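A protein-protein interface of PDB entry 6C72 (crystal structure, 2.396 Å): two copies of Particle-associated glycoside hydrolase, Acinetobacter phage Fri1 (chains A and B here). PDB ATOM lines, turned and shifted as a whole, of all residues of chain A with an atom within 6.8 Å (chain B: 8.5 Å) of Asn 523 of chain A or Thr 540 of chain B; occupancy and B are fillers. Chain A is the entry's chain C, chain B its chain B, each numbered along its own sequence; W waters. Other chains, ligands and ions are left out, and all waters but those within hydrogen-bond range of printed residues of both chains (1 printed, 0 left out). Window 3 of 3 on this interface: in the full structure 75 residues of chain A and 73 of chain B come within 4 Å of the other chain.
No position is printed for both chains. Of the 16 pairs that touch across the chains among the printed residues, none has its exchanged pair printed and touching as well.
N of Arg 508 of chain B sits close to O of Ser 536 of chain B, 3.3 Å away. N of Arg 508 of chain B is in hydrogen-bond range of O of Asp 537 of chain B, 3.0 Å away. The side-chain amide oxygen (OD1) of Asn 538 of chain B lies within hydrogen-bond range of the guanidinium group (NE) of Arg 508 of chain B (2.8 Å). O of Asn 535 of chain B lies within hydrogen-bond range of N of Ile 542 of chain B, 3.0 Å away. The backbone NH (N) of Ser 539 of chain B lies within hydrogen-bond range of the side-chain carboxylate (OD1) of Asp 537 of chain B (2.8 Å). The backbone carbonyl oxygen (O) of Tyr 554 of chain A sits at hydrogen-bond distance from the backbone NH (N) of Lys 527 of chain A, 3.0 Å away.
OD2 of Asp 537 of chain B sits close to N of Asn 523 of chain A, 3.4 Å away. The side-chain carboxylate (OD2) of Asp 537 of chain B sits at hydrogen-bond distance from the backbone NH (N) of Ala 524 of chain A (3.4 Å). The side-chain carboxylate (OD2) of Asp 537 of chain B sits at hydrogen-bond distance from the backbone NH (N) of Gly 525 of chain A (2.8 Å). OD2 of Asp 537 of chain B lies within salt-bridge range of NZ of Lys 527 of chain A, at 2.5 Å. N of Asn 538 of chain B is in hydrogen-bond range of O of Thr 521 of chain A (2.9 Å). ND2 of Asn 538 of chain B lies within hydrogen-bond range of OG1 of Thr 522 of chain A, 3.1 Å away. OD1 of Asn 523 of chain A sits at hydrogen-bond distance from OG of Ser 539 of chain B (2.6 Å). The side-chain amide oxygen of Asn 523 of chain A sits close to the side-chain hydroxyl of Thr 540 of chain B (3.5 Å).
Printed residues of chain A that touch a printed residue of chain B: Ala 520, Thr 521, Thr 522, Asn 523, Ala 524, Gly 525, Ser 526 and Lys 527. Along chain A the printed residues that touch a printed residue of chain B span positions 520 to 527.
Of the printed residues of chain B, Ala 520 of chain A touches Arg 508 (3.6 Å) and Asn 538 (3.2 Å). Asn 523 of chain A touches just these residues of chain B: Asp 537, Ser 539 and Thr 540. Of the printed residues of chain B, Ser 526 of chain A touches Asn 535 (3.6 Å). Of the printed residues of chain A, Arg 508 of chain B touches Ala 520. Ser 509 of chain B touches none of the printed residues of chain A. Of the printed residues of chain A, Ser 539 of chain B touches Thr 522 (3.4 Å) and Asn 523 (2.6 Å). Thr 540 of chain B touches two residues of chain A. Of the printed residues of chain A, Ile 542 of chain B touches Lys 527. Gly 562 of chain B touches none of the printed residues of chain A. The nearest printed residue of chain B that does not touch Gly 525 of chain A is Asn 538 of chain B (5.9 Å).
Water W1 bridges the backbone carbonyl oxygen (O) of Ser 536 of chain B (2.6 Å) and the backbone carbonyl oxygen (O) of Ser 526 of chain A (2.9 Å).
Among the printed residues, pairs that only touch across the chains: Ala 520 of chain A with Arg 508 of chain B, Ala 520 of chain A with Asn 538 of chain B, Thr 521 of chain A with Asp 537 of chain B, Thr 522 of chain A with Ser 539 of chain B, Ser 526 of chain A with Asn 535 of chain B, Lys 527 of chain A with Asn 535 of chain B, Lys 527 of chain A with Thr 540 of chain B and Lys 527 of chain A with Ile 542 of chain B.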
ATOM      1  N   ALA A 520      -3.482 -22.748   6.343  1.00  0.00           N
ATOM      2  CA  ALA A 520      -2.043 -22.541   6.418  1.00  0.00           C
ATOM      3  C   ALA A 520      -1.360 -23.446   7.437  1.00  0.00           C
ATOM      4  O   ALA A 520      -0.139 -23.344   7.601  1.00  0.00           O
ATOM      5  CB  ALA A 520      -1.729 -21.071   6.737  1.00  0.00           C
ATOM      6  N   THR A 521      -2.100 -24.307   8.135  1.00  0.00           N
ATOM      7  CA  THR A 521      -1.465 -25.222   9.075  1.00  0.00           C
ATOM      8  C   THR A 521      -0.702 -26.306   8.324  1.00  0.00           C
ATOM      9  O   THR A 521      -1.132 -26.766   7.262  1.00  0.00           O
ATOM     10  CB  THR A 521      -2.499 -25.868   9.998  1.00  0.00           C
ATOM     11  OG1 THR A 521      -3.233 -24.846  10.678  1.00  0.00           O
ATOM     12  CG2 THR A 521      -1.819 -26.739  11.039  1.00  0.00           C
ATOM     13  N   THR A 522       0.438 -26.714   8.886  1.00  0.00           N
ATOM     14  CA  THR A 522       1.203 -27.823   8.333  1.00  0.00           C
ATOM     15  C   THR A 522       0.611 -29.149   8.798  1.00  0.00           C
ATOM     16  O   THR A 522       0.365 -29.346   9.994  1.00  0.00           O
ATOM     17  CB  THR A 522       2.669 -27.719   8.762  1.00  0.00           C
ATOM     18  OG1 THR A 522       3.216 -26.467   8.325  1.00  0.00           O
ATOM     19  CG2 THR A 522       3.500 -28.868   8.198  1.00  0.00           C
ATOM     20  N   ASN A 523       0.375 -30.051   7.840  1.00  0.00           N
ATOM     21  CA  ASN A 523      -0.063 -31.428   8.069  1.00  0.00           C
ATOM     22  C   ASN A 523      -1.513 -31.551   8.537  1.00  0.00           C
ATOM     23  O   ASN A 523      -2.248 -32.413   8.047  1.00  0.00           O
ATOM     24  CB  ASN A 523       0.856 -32.123   9.087  1.00  0.00           C
ATOM     25  CG  ASN A 523       2.289 -32.264   8.592  1.00  0.00           C
ATOM     26  OD1 ASN A 523       2.553 -32.288   7.388  1.00  0.00           O
ATOM     27  ND2 ASN A 523       3.226 -32.357   9.530  1.00  0.00           N
ATOM     28  N   ALA A 524      -1.934 -30.721   9.492  1.00  0.00           N
ATOM     29  CA  ALA A 524      -3.223 -30.878  10.154  1.00  0.00           C
ATOM     30  C   ALA A 524      -4.275 -29.860   9.701  1.00  0.00           C
ATOM     31  O   ALA A 524      -5.269 -29.645  10.406  1.00  0.00           O
ATOM     32  CB  ALA A 524      -3.029 -30.797  11.670  1.00  0.00           C
ATOM     33  N   GLY A 525      -4.095 -29.242   8.539  1.00  0.00           N
ATOM     34  CA  GLY A 525      -5.058 -28.281   8.045  1.00  0.00           C
ATOM     35  C   GLY A 525      -6.304 -28.941   7.492  1.00  0.00           C
ATOM     36  O   GLY A 525      -6.426 -30.160   7.411  1.00  0.00           O
ATOM     37  N   SER A 526      -7.245 -28.101   7.080  1.00  0.00           N
ATOM     38  CA  SER A 526      -8.520 -28.593   6.580  1.00  0.00           C
ATOM     39  C   SER A 526      -8.359 -29.300   5.237  1.00  0.00           C
ATOM     40  O   SER A 526      -7.509 -28.940   4.420  1.00  0.00           O
ATOM     41  CB  SER A 526      -9.499 -27.431   6.464  1.00  0.00           C
ATOM     42  OG  SER A 526      -8.874 -26.330   5.835  1.00  0.00           O
ATOM     43  N   LYS A 527      -9.159 -30.346   5.032  1.00  0.00           N
ATOM     44  CA  LYS A 527      -9.201 -31.074   3.765  1.00  0.00           C
ATOM     45  C   LYS A 527     -10.655 -31.373   3.458  1.00  0.00           C
ATOM     46  O   LYS A 527     -11.287 -32.158   4.171  1.00  0.00           O
ATOM     47  CB  LYS A 527      -8.388 -32.372   3.804  1.00  0.00           C
ATOM     48  CG  LYS A 527      -6.898 -32.193   3.655  1.00  0.00           C
ATOM     49  CD  LYS A 527      -6.280 -32.194   4.999  1.00  0.00           C
ATOM     50  CE  LYS A 527      -4.774 -31.991   4.941  1.00  0.00           C
ATOM     51  NZ  LYS A 527      -4.240 -31.861   6.332  1.00  0.00           N
ATOM     52  N   TYR A 554     -10.386 -33.948   9.391  1.00  0.00           N
ATOM     53  CA  TYR A 554     -10.046 -32.584   9.004  1.00  0.00           C
ATOM     54  C   TYR A 554     -11.060 -31.930   8.064  1.00  0.00           C
ATOM     55  O   TYR A 554     -10.748 -30.894   7.464  1.00  0.00           O
ATOM     56  CB  TYR A 554      -8.662 -32.558   8.360  1.00  0.00           C
ATOM     57  CG  TYR A 554      -7.531 -32.968   9.263  1.00  0.00           C
ATOM     58  CD1 TYR A 554      -7.572 -32.693  10.622  1.00  0.00           C
ATOM     59  CD2 TYR A 554      -6.395 -33.591   8.749  1.00  0.00           C
ATOM     60  CE1 TYR A 554      -6.526 -33.047  11.456  1.00  0.00           C
ATOM     61  CE2 TYR A 554      -5.338 -33.963   9.571  1.00  0.00           C
ATOM     62  CZ  TYR A 554      -5.406 -33.682  10.931  1.00  0.00           C
ATOM     63  OH  TYR A 554      -4.360 -34.036  11.764  1.00  0.00           O
ATOM     64  N   PRO B 506      -1.007 -25.313  -6.182  1.00  0.00           N
ATOM     65  CA  PRO B 506      -0.354 -24.701  -5.023  1.00  0.00           C
ATOM     66  C   PRO B 506      -0.809 -25.362  -3.729  1.00  0.00           C
ATOM     67  O   PRO B 506      -1.746 -26.162  -3.697  1.00  0.00           O
ATOM     68  CB  PRO B 506      -0.807 -23.238  -5.091  1.00  0.00           C
ATOM     69  CG  PRO B 506      -2.119 -23.293  -5.791  1.00  0.00           C
ATOM     70  CD  PRO B 506      -2.035 -24.432  -6.768  1.00  0.00           C
ATOM     71  N   LEU B 507      -0.093 -25.036  -2.657  1.00  0.00           N
ATOM     72  CA  LEU B 507      -0.503 -25.444  -1.323  1.00  0.00           C
ATOM     73  C   LEU B 507      -1.687 -24.590  -0.871  1.00  0.00           C
ATOM     74  O   LEU B 507      -2.113 -23.665  -1.562  1.00  0.00           O
ATOM     75  CB  LEU B 507       0.674 -25.328  -0.353  1.00  0.00           C
ATOM     76  CG  LEU B 507       1.826 -26.332  -0.475  1.00  0.00           C
ATOM     77  CD1 LEU B 507       3.041 -25.840   0.309  1.00  0.00           C
ATOM     78  CD2 LEU B 507       1.402 -27.695   0.038  1.00  0.00           C
ATOM     79  N   ARG B 508      -2.224 -24.909   0.308  1.00  0.00           N
ATOM     80  CA  ARG B 508      -3.239 -24.083   0.970  1.00  0.00           C
ATOM     81  C   ARG B 508      -4.400 -23.746   0.040  1.00  0.00           C
ATOM     82  O   ARG B 508      -4.875 -22.611  -0.007  1.00  0.00           O
ATOM     83  CB  ARG B 508      -2.635 -22.794   1.517  1.00  0.00           C
ATOM     84  CG  ARG B 508      -1.351 -22.960   2.277  1.00  0.00           C
ATOM     85  CD  ARG B 508      -0.914 -21.616   2.810  1.00  0.00           C
ATOM     86  NE  ARG B 508       0.354 -21.693   3.516  1.00  0.00           N
ATOM     87  CZ  ARG B 508       0.905 -20.667   4.163  1.00  0.00           C
ATOM     88  NH1 ARG B 508       0.284 -19.494   4.190  1.00  0.00           N
ATOM     89  NH2 ARG B 508       2.074 -20.813   4.782  1.00  0.00           N
ATOM     90  N   SER B 509      -4.863 -24.736  -0.710  1.00  0.00           N
ATOM     91  CA  SER B 509      -5.854 -24.430  -1.724  1.00  0.00           C
ATOM     92  C   SER B 509      -6.646 -25.677  -2.073  1.00  0.00           C
ATOM     93  O   SER B 509      -6.161 -26.802  -1.925  1.00  0.00           O
ATOM     94  CB  SER B 509      -5.180 -23.841  -2.967  1.00  0.00           C
ATOM     95  OG  SER B 509      -4.255 -24.756  -3.539  1.00  0.00           O
ATOM     96  N   VAL B 534      -8.405 -31.521  -5.781  1.00  0.00           N
ATOM     97  CA  VAL B 534      -7.255 -31.517  -4.888  1.00  0.00           C
ATOM     98  C   VAL B 534      -7.550 -30.573  -3.738  1.00  0.00           C
ATOM     99  O   VAL B 534      -8.071 -29.476  -3.950  1.00  0.00           O
ATOM    100  CB  VAL B 534      -5.967 -31.031  -5.579  1.00  0.00           C
ATOM    101  CG1 VAL B 534      -4.758 -31.373  -4.729  1.00  0.00           C
ATOM    102  CG2 VAL B 534      -5.844 -31.565  -6.970  1.00  0.00           C
ATOM    103  N   ASN B 535      -7.152 -30.955  -2.533  1.00  0.00           N
ATOM    104  CA  ASN B 535      -7.140 -30.009  -1.426  1.00  0.00           C
ATOM    105  C   ASN B 535      -5.826 -30.183  -0.679  1.00  0.00           C
ATOM    106  O   ASN B 535      -5.393 -31.312  -0.433  1.00  0.00           O
ATOM    107  CB  ASN B 535      -8.347 -30.216  -0.501  1.00  0.00           C
ATOM    108  CG  ASN B 535      -8.698 -28.971   0.289  1.00  0.00           C
ATOM    109  OD1 ASN B 535      -9.385 -29.038   1.308  1.00  0.00           O
ATOM    110  ND2 ASN B 535      -8.221 -27.823  -0.173  1.00  0.00           N
ATOM    111  N   SER B 536      -5.167 -29.071  -0.364  1.00  0.00           N
ATOM    112  CA  SER B 536      -3.910 -29.106   0.369  1.00  0.00           C
ATOM    113  C   SER B 536      -3.927 -28.098   1.505  1.00  0.00           C
ATOM    114  O   SER B 536      -4.492 -27.007   1.381  1.00  0.00           O
ATOM    115  CB  SER B 536      -2.700 -28.796  -0.519  1.00  0.00           C
ATOM    116  OG  SER B 536      -2.636 -29.660  -1.630  1.00  0.00           O
ATOM    117  N   ASP B 537      -3.280 -28.458   2.608  1.00  0.00           N
ATOM    118  CA  ASP B 537      -2.979 -27.432   3.594  1.00  0.00           C
ATOM    119  C   ASP B 537      -1.566 -26.936   3.328  1.00  0.00           C
ATOM    120  O   ASP B 537      -1.124 -26.917   2.173  1.00  0.00           O
ATOM    121  CB  ASP B 537      -3.158 -27.961   5.015  1.00  0.00           C
ATOM    122  CG  ASP B 537      -2.289 -29.183   5.319  1.00  0.00           C
ATOM    123  OD1 ASP B 537      -1.260 -29.427   4.641  1.00  0.00           O
ATOM    124  OD2 ASP B 537      -2.670 -29.934   6.236  1.00  0.00           O
ATOM    125  N   ASN B 538      -0.828 -26.587   4.373  1.00  0.00           N
ATOM    126  CA  ASN B 538       0.509 -26.064   4.139  1.00  0.00           C
ATOM    127  C   ASN B 538       1.506 -27.141   3.713  1.00  0.00           C
ATOM    128  O   ASN B 538       2.633 -26.796   3.352  1.00  0.00           O
ATOM    129  CB  ASN B 538       1.026 -25.362   5.391  1.00  0.00           C
ATOM    130  CG  ASN B 538       2.202 -24.460   5.101  1.00  0.00           C
ATOM    131  OD1 ASN B 538       2.204 -23.724   4.115  1.00  0.00           O
ATOM    132  ND2 ASN B 538       3.235 -24.545   5.935  1.00  0.00           N
ATOM    133  N   SER B 539       1.132 -28.423   3.721  1.00  0.00           N
ATOM    134  CA  SER B 539       2.091 -29.442   3.313  1.00  0.00           C
ATOM    135  C   SER B 539       1.442 -30.720   2.789  1.00  0.00           C
ATOM    136  O   SER B 539       2.062 -31.442   2.005  1.00  0.00           O
ATOM    137  CB  SER B 539       3.025 -29.784   4.468  1.00  0.00           C
ATOM    138  OG  SER B 539       2.328 -30.471   5.480  1.00  0.00           O
ATOM    139  N   THR B 540       0.212 -31.022   3.195  1.00  0.00           N
ATOM    140  CA  THR B 540      -0.426 -32.298   2.884  1.00  0.00           C
ATOM    141  C   THR B 540      -1.497 -32.122   1.812  1.00  0.00           C
ATOM    142  O   THR B 540      -2.206 -31.112   1.795  1.00  0.00           O
ATOM    143  CB  THR B 540      -1.028 -32.905   4.153  1.00  0.00           C
ATOM    144  OG1 THR B 540       0.015 -33.050   5.123  1.00  0.00           O
ATOM    145  CG2 THR B 540      -1.643 -34.253   3.881  1.00  0.00           C
ATOM    146  N   THR B 541      -1.636 -33.132   0.941  1.00  0.00           N
ATOM    147  CA  THR B 541      -2.476 -33.066  -0.256  1.00  0.00           C
ATOM    148  C   THR B 541      -3.318 -34.328  -0.393  1.00  0.00           C
ATOM    149  O   THR B 541      -2.788 -35.440  -0.293  1.00  0.00           O
ATOM    150  CB  THR B 541      -1.617 -32.912  -1.514  1.00  0.00           C
ATOM    151  OG1 THR B 541      -1.000 -31.621  -1.530  1.00  0.00           O
ATOM    152  CG2 THR B 541      -2.457 -33.101  -2.768  1.00  0.00           C
ATOM    153  N   ILE B 542      -4.618 -34.159  -0.645  1.00  0.00           N
ATOM    154  CA  ILE B 542      -5.526 -35.261  -0.947  1.00  0.00           C
ATOM    155  C   ILE B 542      -6.139 -35.012  -2.321  1.00  0.00           C
ATOM    156  O   ILE B 542      -6.498 -33.875  -2.643  1.00  0.00           O
ATOM    157  CB  ILE B 542      -6.626 -35.404   0.128  1.00  0.00           C
ATOM    158  CG1 ILE B 542      -5.983 -35.574   1.513  1.00  0.00           C
ATOM    159  CG2 ILE B 542      -7.516 -36.592  -0.177  1.00  0.00           C
ATOM    160  CD1 ILE B 542      -6.957 -35.892   2.687  1.00  0.00           C
ATOM    161  N   THR B 543      -6.279 -36.066  -3.121  1.00  0.00           N
ATOM    162  CA  THR B 543      -6.876 -35.946  -4.443  1.00  0.00           C
ATOM    163  C   THR B 543      -8.108 -36.835  -4.554  1.00  0.00           C
ATOM    164  O   THR B 543      -8.311 -37.754  -3.757  1.00  0.00           O
ATOM    165  CB  THR B 543      -5.888 -36.312  -5.563  1.00  0.00           C
ATOM    166  OG1 THR B 543      -5.561 -37.706  -5.483  1.00  0.00           O
ATOM    167  CG2 THR B 543      -4.625 -35.485  -5.467  1.00  0.00           C
ATOM    168  N   GLY B 562       2.490 -36.304  -5.930  1.00  0.00           N
ATOM    169  CA  GLY B 562       2.327 -35.170  -5.040  1.00  0.00           C
ATOM    170  C   GLY B 562       1.281 -34.216  -5.597  1.00  0.00           C
ATOM    171  O   GLY B 562       0.118 -34.582  -5.817  1.00  0.00           O
ATOM    172  N   ARG B 563       1.689 -32.972  -5.828  1.00  0.00           N
ATOM    173  CA  ARG B 563       0.808 -31.935  -6.348  1.00  0.00           C
ATOM    174  C   ARG B 563       0.976 -31.706  -7.850  1.00  0.00           C
ATOM    175  O   ARG B 563       0.358 -30.789  -8.401  1.00  0.00           O
ATOM    176  CB  ARG B 563       1.026 -30.632  -5.571  1.00  0.00           C
ATOM    177  CG  ARG B 563       0.212 -30.534  -4.271  1.00  0.00           C
ATOM    178  CD  ARG B 563       0.889 -29.692  -3.185  1.00  0.00           C
ATOM    179  NE  ARG B 563       1.535 -28.499  -3.719  1.00  0.00           N
ATOM    180  CZ  ARG B 563       2.823 -28.229  -3.583  1.00  0.00           C
ATOM    181  NH1 ARG B 563       3.600 -29.064  -2.905  1.00  0.00           N
ATOM    182  NH2 ARG B 563       3.332 -27.125  -4.118  1.00  0.00           N
HETATM  183  O   HOH W   1      -6.322 -26.587   3.232  1.00  0.00           O
